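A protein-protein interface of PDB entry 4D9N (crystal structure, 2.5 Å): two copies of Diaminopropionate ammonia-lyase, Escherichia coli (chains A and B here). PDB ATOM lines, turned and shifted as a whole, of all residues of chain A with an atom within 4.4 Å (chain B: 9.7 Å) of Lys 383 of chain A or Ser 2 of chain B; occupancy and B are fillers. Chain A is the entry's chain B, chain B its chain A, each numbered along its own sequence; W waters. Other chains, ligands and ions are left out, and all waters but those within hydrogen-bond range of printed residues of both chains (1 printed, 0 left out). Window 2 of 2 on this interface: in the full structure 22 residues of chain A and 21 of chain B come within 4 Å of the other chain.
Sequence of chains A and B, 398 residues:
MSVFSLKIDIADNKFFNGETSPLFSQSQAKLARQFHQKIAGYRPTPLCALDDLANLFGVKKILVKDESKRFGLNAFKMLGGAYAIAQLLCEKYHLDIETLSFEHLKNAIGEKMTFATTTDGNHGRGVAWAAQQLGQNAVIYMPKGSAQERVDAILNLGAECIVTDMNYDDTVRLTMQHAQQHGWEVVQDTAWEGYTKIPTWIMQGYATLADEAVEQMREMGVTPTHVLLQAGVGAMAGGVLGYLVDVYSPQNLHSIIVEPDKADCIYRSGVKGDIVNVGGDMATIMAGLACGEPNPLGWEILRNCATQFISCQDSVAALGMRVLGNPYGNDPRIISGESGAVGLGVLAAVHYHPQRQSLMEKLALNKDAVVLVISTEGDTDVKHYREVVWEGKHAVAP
N of Ser 2 of chain B sits close to OE2 of Glu 387 of chain A (3.3 Å).
The backbone NH (N) of Ser 2 of chain B sits at hydrogen-bond distance from the side-chain carboxylate (OE1) of Glu 391 of chain A (2.8 Å).
N of Val 396 of chain B is in hydrogen-bond range of O of Glu 391 of chain A, at 3.0 Å.
N of Phe 4 of chain B sits at hydrogen-bond distance from O of Tyr 352 of chain B (2.9 Å).
N of Lys 383 of chain A sits close to OD1 of Asp 381 of chain A, at 3.3 Å.
NZ of Lys 383 of chain A is in salt-bridge range of OE2 of Glu 387 of chain A.
The backbone carbonyl oxygen (O) of Arg 386 of chain A sits at hydrogen-bond distance from the backbone NH (N) of Glu 391 of chain A (3.4 Å).
Among the printed residues, pairs that only touch across the chains: Lys 383 of chain A with Ser 2 of chain B (3.5 Å), Glu 391 of chain A with Phe 4 of chain B (3.5 Å) and Arg 386 of chain A with Tyr 328 of chain B (3.6 Å).
No residue of chain B comes within 4 Å of Asp 381 of chain A.
No residue of chain B comes within 4 Å of Val 382 of chain A.
Printed residues of chain B within 4 Å of Arg 386 of chain A: Tyr 328.
Of the printed residues of chain B, Glu 387 of chain A touches Ser 2.
Printed residues of chain A within 4 Å of Phe 4 of chain B: Glu 391.
Printed residues of chain A within 4 Å of Tyr 328 of chain B: Arg 386 (3.6 Å).
Of the printed residues of chain A, Val 396 of chain B touches Glu 391.
The nearest residue of chain B that does not touch Lys 383 of chain A is Val 3 of chain B (6.2 Å).
The nearest printed residue of chain A that does not touch Phe 4 of chain B is Glu 387 of chain A (7.0 Å).
Hydrophobic or aromatic side chains of chain B within 4 Å of the printed part of chain A: Phe 4, Tyr 328 and Val 396.
Of the 8 printed residues of chain A, 4 touch a printed residue of chain B.
Among the printed residues, 6 pairs touch across the chains.
No position is printed for both chains.
Of the 6 pairs that touch across the chains among the printed residues, none has its exchanged pair printed and touching as well.
Water W1 lies within hydrogen-bond range of OE2 of Glu 391 of chain A (2.7 Å), OH of Tyr 352 of chain B (3.0 Å) and O of Arg 386 of chain A (3.3 Å).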
ATOM      1  N   ASP A 381      30.026  11.521  31.023  1.00  0.00           N
ATOM      2  CA  ASP A 381      29.817  12.774  31.733  1.00  0.00           C
ATOM      3  C   ASP A 381      29.266  13.806  30.749  1.00  0.00           C
ATOM      4  O   ASP A 381      30.033  14.508  30.084  1.00  0.00           O
ATOM      5  CB  ASP A 381      31.126  13.261  32.371  1.00  0.00           C
ATOM      6  CG  ASP A 381      30.933  14.481  33.266  1.00  0.00           C
ATOM      7  OD1 ASP A 381      29.831  15.072  33.269  1.00  0.00           O
ATOM      8  OD2 ASP A 381      31.895  14.854  33.969  1.00  0.00           O
ATOM      9  N   VAL A 382      27.936  13.886  30.659  1.00  0.00           N
ATOM     10  CA  VAL A 382      27.264  14.785  29.704  1.00  0.00           C
ATOM     11  C   VAL A 382      27.637  16.254  29.919  1.00  0.00           C
ATOM     12  O   VAL A 382      27.741  17.016  28.956  1.00  0.00           O
ATOM     13  CB  VAL A 382      25.720  14.614  29.675  1.00  0.00           C
ATOM     14  CG1 VAL A 382      25.332  13.223  29.194  1.00  0.00           C
ATOM     15  CG2 VAL A 382      25.089  14.906  31.030  1.00  0.00           C
ATOM     16  N   LYS A 383      27.849  16.628  31.181  1.00  0.00           N
ATOM     17  CA  LYS A 383      28.264  17.980  31.548  1.00  0.00           C
ATOM     18  C   LYS A 383      29.619  18.312  30.934  1.00  0.00           C
ATOM     19  O   LYS A 383      29.764  19.318  30.237  1.00  0.00           O
ATOM     20  CB  LYS A 383      28.313  18.129  33.074  1.00  0.00           C
ATOM     21  CG  LYS A 383      28.440  19.562  33.565  1.00  0.00           C
ATOM     22  CD  LYS A 383      28.422  19.622  35.087  1.00  0.00           C
ATOM     23  CE  LYS A 383      28.640  21.041  35.593  1.00  0.00           C
ATOM     24  NZ  LYS A 383      29.994  21.564  35.245  1.00  0.00           N
ATOM     25  N   HIS A 384      30.600  17.448  31.188  1.00  0.00           N
ATOM     26  CA  HIS A 384      31.955  17.622  30.674  1.00  0.00           C
ATOM     27  C   HIS A 384      32.024  17.529  29.171  1.00  0.00           C
ATOM     28  O   HIS A 384      32.753  18.295  28.536  1.00  0.00           O
ATOM     29  CB  HIS A 384      32.892  16.604  31.318  1.00  0.00           C
ATOM     30  CG  HIS A 384      34.287  16.611  30.747  1.00  0.00           C
ATOM     31  ND1 HIS A 384      35.193  17.551  31.068  1.00  0.00           N
ATOM     32  CD2 HIS A 384      34.910  15.752  29.845  1.00  0.00           C
ATOM     33  CE1 HIS A 384      36.341  17.307  30.408  1.00  0.00           C
ATOM     34  NE2 HIS A 384      36.166  16.205  29.661  1.00  0.00           N
ATOM     35  N   TYR A 385      31.267  16.596  28.593  1.00  0.00           N
ATOM     36  CA  TYR A 385      31.268  16.378  27.142  1.00  0.00           C
ATOM     37  C   TYR A 385      30.808  17.608  26.360  1.00  0.00           C
ATOM     38  O   TYR A 385      31.394  17.957  25.333  1.00  0.00           O
ATOM     39  CB  TYR A 385      30.401  15.170  26.762  1.00  0.00           C
ATOM     40  CG  TYR A 385      30.321  14.940  25.268  1.00  0.00           C
ATOM     41  CD1 TYR A 385      31.313  14.220  24.603  1.00  0.00           C
ATOM     42  CD2 TYR A 385      29.264  15.457  24.513  1.00  0.00           C
ATOM     43  CE1 TYR A 385      31.253  14.016  23.235  1.00  0.00           C
ATOM     44  CE2 TYR A 385      29.198  15.257  23.143  1.00  0.00           C
ATOM     45  CZ  TYR A 385      30.195  14.537  22.510  1.00  0.00           C
ATOM     46  OH  TYR A 385      30.144  14.327  21.154  1.00  0.00           O
ATOM     47  N   ARG A 386      29.752  18.251  26.844  1.00  0.00           N
ATOM     48  CA  ARG A 386      29.184  19.403  26.160  1.00  0.00           C
ATOM     49  C   ARG A 386      29.999  20.669  26.405  1.00  0.00           C
ATOM     50  O   ARG A 386      29.976  21.592  25.591  1.00  0.00           O
ATOM     51  CB  ARG A 386      27.711  19.595  26.533  1.00  0.00           C
ATOM     52  CG  ARG A 386      26.797  18.476  26.042  1.00  0.00           C
ATOM     53  CD  ARG A 386      26.748  18.383  24.521  1.00  0.00           C
ATOM     54  NE  ARG A 386      26.006  17.205  24.066  1.00  0.00           N
ATOM     55  CZ  ARG A 386      25.806  16.881  22.790  1.00  0.00           C
ATOM     56  NH1 ARG A 386      26.292  17.643  21.815  1.00  0.00           N
ATOM     57  NH2 ARG A 386      25.116  15.792  22.485  1.00  0.00           N
ATOM     58  N   GLU A 387      30.731  20.703  27.517  1.00  0.00           N
ATOM     59  CA  GLU A 387      31.673  21.789  27.779  1.00  0.00           C
ATOM     60  C   GLU A 387      32.830  21.748  26.786  1.00  0.00           C
ATOM     61  O   GLU A 387      33.352  22.788  26.382  1.00  0.00           O
ATOM     62  CB  GLU A 387      32.201  21.717  29.210  1.00  0.00           C
ATOM     63  CG  GLU A 387      31.253  22.304  30.242  1.00  0.00           C
ATOM     64  CD  GLU A 387      31.624  21.942  31.666  1.00  0.00           C
ATOM     65  OE1 GLU A 387      32.668  21.285  31.871  1.00  0.00           O
ATOM     66  OE2 GLU A 387      30.863  22.313  32.585  1.00  0.00           O
ATOM     67  N   GLU A 391      31.345  24.481  24.467  1.00  0.00           N
ATOM     68  CA  GLU A 391      31.947  25.643  25.123  1.00  0.00           C
ATOM     69  C   GLU A 391      33.420  25.802  24.750  1.00  0.00           C
ATOM     70  O   GLU A 391      34.016  26.864  24.961  1.00  0.00           O
ATOM     71  CB  GLU A 391      31.775  25.561  26.644  1.00  0.00           C
ATOM     72  CG  GLU A 391      30.333  25.410  27.110  1.00  0.00           C
ATOM     73  CD  GLU A 391      30.192  25.350  28.623  1.00  0.00           C
ATOM     74  OE1 GLU A 391      31.097  25.835  29.337  1.00  0.00           O
ATOM     75  OE2 GLU A 391      29.166  24.825  29.103  1.00  0.00           O
ATOM     76  N   SER B   2      30.501  25.573  32.064  1.00  0.00           N
ATOM     77  CA  SER B   2      29.139  25.228  32.560  1.00  0.00           C
ATOM     78  C   SER B   2      28.262  26.462  32.510  1.00  0.00           C
ATOM     79  O   SER B   2      27.555  26.684  31.530  1.00  0.00           O
ATOM     80  CB  SER B   2      29.209  24.686  33.989  1.00  0.00           C
ATOM     81  N   VAL B   3      28.313  27.260  33.573  1.00  0.00           N
ATOM     82  CA  VAL B   3      27.623  28.546  33.624  1.00  0.00           C
ATOM     83  C   VAL B   3      28.623  29.639  33.257  1.00  0.00           C
ATOM     84  O   VAL B   3      29.706  29.720  33.844  1.00  0.00           O
ATOM     85  CB  VAL B   3      27.008  28.811  35.018  1.00  0.00           C
ATOM     86  CG1 VAL B   3      26.297  30.155  35.051  1.00  0.00           C
ATOM     87  CG2 VAL B   3      26.041  27.697  35.395  1.00  0.00           C
ATOM     88  N   PHE B   4      28.264  30.468  32.279  1.00  0.00           N
ATOM     89  CA  PHE B   4      29.160  31.516  31.784  1.00  0.00           C
ATOM     90  C   PHE B   4      28.413  32.731  31.239  1.00  0.00           C
ATOM     91  O   PHE B   4      27.268  32.618  30.789  1.00  0.00           O
ATOM     92  CB  PHE B   4      30.121  30.955  30.726  1.00  0.00           C
ATOM     93  CG  PHE B   4      29.436  30.350  29.529  1.00  0.00           C
ATOM     94  CD1 PHE B   4      29.105  31.133  28.425  1.00  0.00           C
ATOM     95  CD2 PHE B   4      29.144  28.991  29.491  1.00  0.00           C
ATOM     96  CE1 PHE B   4      28.483  30.576  27.318  1.00  0.00           C
ATOM     97  CE2 PHE B   4      28.526  28.429  28.385  1.00  0.00           C
ATOM     98  CZ  PHE B   4      28.192  29.222  27.298  1.00  0.00           C
ATOM     99  N   SER B   5      29.073  33.887  31.274  1.00  0.00           N
ATOM    100  CA  SER B   5      28.473  35.138  30.814  1.00  0.00           C
ATOM    101  C   SER B   5      29.086  35.644  29.514  1.00  0.00           C
ATOM    102  O   SER B   5      30.254  36.044  29.476  1.00  0.00           O
ATOM    103  CB  SER B   5      28.576  36.218  31.895  1.00  0.00           C
ATOM    104  OG  SER B   5      27.662  35.976  32.947  1.00  0.00           O
ATOM    105  N   LEU B   6      28.290  35.612  28.449  1.00  0.00           N
ATOM    106  CA  LEU B   6      28.656  36.236  27.182  1.00  0.00           C
ATOM    107  C   LEU B   6      27.781  37.459  26.974  1.00  0.00           C
ATOM    108  O   LEU B   6      26.585  37.427  27.271  1.00  0.00           O
ATOM    109  CB  LEU B   6      28.494  35.258  26.011  1.00  0.00           C
ATOM    110  CG  LEU B   6      29.314  33.961  25.999  1.00  0.00           C
ATOM    111  CD1 LEU B   6      29.026  33.177  24.727  1.00  0.00           C
ATOM    112  CD2 LEU B   6      30.809  34.223  26.139  1.00  0.00           C
ATOM    113  N   LEU B  56      16.039  21.009  26.283  1.00  0.00           N
ATOM    114  CA  LEU B  56      17.142  21.433  27.143  1.00  0.00           C
ATOM    115  C   LEU B  56      17.077  22.933  27.442  1.00  0.00           C
ATOM    116  O   LEU B  56      17.344  23.357  28.567  1.00  0.00           O
ATOM    117  CB  LEU B  56      18.496  21.063  26.523  1.00  0.00           C
ATOM    118  CG  LEU B  56      19.779  21.370  27.310  1.00  0.00           C
ATOM    119  CD1 LEU B  56      19.985  20.400  28.468  1.00  0.00           C
ATOM    120  CD2 LEU B  56      20.989  21.364  26.386  1.00  0.00           C
ATOM    121  N   LEU B 319      29.775  29.684  19.463  1.00  0.00           N
ATOM    122  CA  LEU B 319      28.979  28.784  20.301  1.00  0.00           C
ATOM    123  C   LEU B 319      27.865  28.119  19.491  1.00  0.00           C
ATOM    124  O   LEU B 319      27.647  26.912  19.609  1.00  0.00           O
ATOM    125  CB  LEU B 319      28.405  29.541  21.505  1.00  0.00           C
ATOM    126  CG  LEU B 319      27.420  28.841  22.449  1.00  0.00           C
ATOM    127  CD1 LEU B 319      28.069  27.676  23.188  1.00  0.00           C
ATOM    128  CD2 LEU B 319      26.845  29.849  23.432  1.00  0.00           C
ATOM    129  N   TYR B 328      22.362  18.023  20.252  1.00  0.00           N
ATOM    130  CA  TYR B 328      22.007  17.367  21.503  1.00  0.00           C
ATOM    131  C   TYR B 328      21.016  16.241  21.223  1.00  0.00           C
ATOM    132  O   TYR B 328      20.204  16.338  20.299  1.00  0.00           O
ATOM    133  CB  TYR B 328      21.399  18.394  22.464  1.00  0.00           C
ATOM    134  CG  TYR B 328      21.400  17.996  23.928  1.00  0.00           C
ATOM    135  CD1 TYR B 328      22.585  17.972  24.666  1.00  0.00           C
ATOM    136  CD2 TYR B 328      20.212  17.670  24.583  1.00  0.00           C
ATOM    137  CE1 TYR B 328      22.590  17.621  26.008  1.00  0.00           C
ATOM    138  CE2 TYR B 328      20.208  17.317  25.925  1.00  0.00           C
ATOM    139  CZ  TYR B 328      21.399  17.296  26.632  1.00  0.00           C
ATOM    140  OH  TYR B 328      21.404  16.947  27.964  1.00  0.00           O
ATOM    141  N   ALA B 348      21.635  29.629  22.972  1.00  0.00           N
ATOM    142  CA  ALA B 348      22.571  28.847  23.778  1.00  0.00           C
ATOM    143  C   ALA B 348      23.286  29.703  24.826  1.00  0.00           C
ATOM    144  O   ALA B 348      23.515  29.250  25.948  1.00  0.00           O
ATOM    145  CB  ALA B 348      23.575  28.126  22.889  1.00  0.00           C
ATOM    146  N   ALA B 349      23.632  30.934  24.456  1.00  0.00           N
ATOM    147  CA  ALA B 349      24.295  31.856  25.377  1.00  0.00           C
ATOM    148  C   ALA B 349      23.372  32.268  26.520  1.00  0.00           C
ATOM    149  O   ALA B 349      23.828  32.487  27.647  1.00  0.00           O
ATOM    150  CB  ALA B 349      24.814  33.078  24.636  1.00  0.00           C
ATOM    151  N   VAL B 350      22.076  32.359  26.222  1.00  0.00           N
ATOM    152  CA  VAL B 350      21.057  32.676  27.224  1.00  0.00           C
ATOM    153  C   VAL B 350      20.898  31.520  28.216  1.00  0.00           C
ATOM    154  O   VAL B 350      20.828  31.739  29.430  1.00  0.00           O
ATOM    155  CB  VAL B 350      19.700  33.023  26.562  1.00  0.00           C
ATOM    156  CG1 VAL B 350      18.581  33.091  27.590  1.00  0.00           C
ATOM    157  CG2 VAL B 350      19.798  34.340  25.802  1.00  0.00           C
ATOM    158  N   HIS B 351      20.866  30.296  27.691  1.00  0.00           N
ATOM    159  CA  HIS B 351      20.663  29.098  28.506  1.00  0.00           C
ATOM    160  C   HIS B 351      21.718  28.887  29.557  1.00  0.00           C
ATOM    161  O   HIS B 351      21.401  28.535  30.692  1.00  0.00           O
ATOM    162  CB  HIS B 351      20.550  27.860  27.624  1.00  0.00           C
ATOM    163  CG  HIS B 351      20.331  26.582  28.398  1.00  0.00           C
ATOM    164  ND1 HIS B 351      21.332  25.732  28.689  1.00  0.00           N
ATOM    165  CD2 HIS B 351      19.178  26.037  28.955  1.00  0.00           C
ATOM    166  CE1 HIS B 351      20.845  24.690  29.389  1.00  0.00           C
ATOM    167  NE2 HIS B 351      19.526  24.879  29.551  1.00  0.00           N
ATOM    168  N   TYR B 352      22.980  29.102  29.192  1.00  0.00           N
ATOM    169  CA  TYR B 352      24.102  28.884  30.107  1.00  0.00           C
ATOM    170  C   TYR B 352      24.476  30.123  30.928  1.00  0.00           C
ATOM    171  O   TYR B 352      25.402  30.077  31.740  1.00  0.00           O
ATOM    172  CB  TYR B 352      25.327  28.377  29.343  1.00  0.00           C
ATOM    173  CG  TYR B 352      25.204  26.965  28.814  1.00  0.00           C
ATOM    174  CD1 TYR B 352      25.264  25.867  29.675  1.00  0.00           C
ATOM    175  CD2 TYR B 352      25.049  26.723  27.448  1.00  0.00           C
ATOM    176  CE1 TYR B 352      25.162  24.571  29.195  1.00  0.00           C
ATOM    177  CE2 TYR B 352      24.945  25.428  26.958  1.00  0.00           C
ATOM    178  CZ  TYR B 352      25.002  24.356  27.833  1.00  0.00           C
ATOM    179  OH  TYR B 352      24.900  23.068  27.355  1.00  0.00           O
ATOM    180  N   HIS B 353      23.758  31.221  30.712  1.00  0.00           N
ATOM    181  CA  HIS B 353      23.989  32.470  31.434  1.00  0.00           C
ATOM    182  C   HIS B 353      23.535  32.341  32.866  1.00  0.00           C
ATOM    183  O   HIS B 353      22.559  31.638  33.139  1.00  0.00           O
ATOM    184  CB  HIS B 353      23.240  33.606  30.742  1.00  0.00           C
ATOM    185  CG  HIS B 353      23.861  34.968  30.948  1.00  0.00           C
ATOM    186  ND1 HIS B 353      23.541  35.761  31.985  1.00  0.00           N
ATOM    187  CD2 HIS B 353      24.803  35.667  30.194  1.00  0.00           C
ATOM    188  CE1 HIS B 353      24.244  36.906  31.908  1.00  0.00           C
ATOM    189  NE2 HIS B 353      25.014  36.849  30.811  1.00  0.00           N
ATOM    190  N   PRO B 354      24.245  33.000  33.809  1.00  0.00           N
ATOM    191  CA  PRO B 354      23.792  33.014  35.206  1.00  0.00           C
ATOM    192  C   PRO B 354      22.402  33.629  35.335  1.00  0.00           C
ATOM    193  O   PRO B 354      21.566  33.119  36.083  1.00  0.00           O
ATOM    194  CB  PRO B 354      24.825  33.903  35.910  1.00  0.00           C
ATOM    195  CG  PRO B 354      26.037  33.845  35.052  1.00  0.00           C
ATOM    196  CD  PRO B 354      25.551  33.664  33.644  1.00  0.00           C
ATOM    197  N   ARG B 356      19.980  33.531  33.342  1.00  0.00           N
ATOM    198  CA  ARG B 356      19.136  32.785  32.405  1.00  0.00           C
ATOM    199  C   ARG B 356      17.650  33.144  32.504  1.00  0.00           C
ATOM    200  O   ARG B 356      17.004  33.397  31.489  1.00  0.00           O
ATOM    201  CB  ARG B 356      19.329  31.280  32.644  1.00  0.00           C
ATOM    202  CG  ARG B 356      18.513  30.351  31.759  1.00  0.00           C
ATOM    203  CD  ARG B 356      18.533  28.938  32.324  1.00  0.00           C
ATOM    204  NE  ARG B 356      17.978  27.951  31.397  1.00  0.00           N
ATOM    205  CZ  ARG B 356      16.705  27.561  31.375  1.00  0.00           C
ATOM    206  NH1 ARG B 356      15.822  28.073  32.224  1.00  0.00           N
ATOM    207  NH2 ARG B 356      16.311  26.653  30.492  1.00  0.00           N
ATOM    208  N   VAL B 396      34.592  29.844  25.153  1.00  0.00           N
ATOM    209  CA  VAL B 396      33.811  30.534  26.171  1.00  0.00           C
ATOM    210  C   VAL B 396      34.681  31.287  27.189  1.00  0.00           C
ATOM    211  O   VAL B 396      34.512  32.495  27.377  1.00  0.00           O
ATOM    212  CB  VAL B 396      32.850  29.542  26.865  1.00  0.00           C
ATOM    213  CG1 VAL B 396      32.524  29.971  28.289  1.00  0.00           C
ATOM    214  CG2 VAL B 396      31.590  29.364  26.028  1.00  0.00           C
ATOM    215  N   ALA B 397      35.609  30.577  27.831  1.00  0.00           N
ATOM    216  CA  ALA B 397      36.458  31.166  28.869  1.00  0.00           C
ATOM    217  C   ALA B 397      37.860  31.464  28.344  1.00  0.00           C
ATOM    218  O   ALA B 397      38.493  30.613  27.712  1.00  0.00           O
ATOM    219  CB  ALA B 397      36.525  30.250  30.084  1.00  0.00           C
HETATM  220  O   HOH W   1      27.852  22.800  27.851  1.00  0.00           O
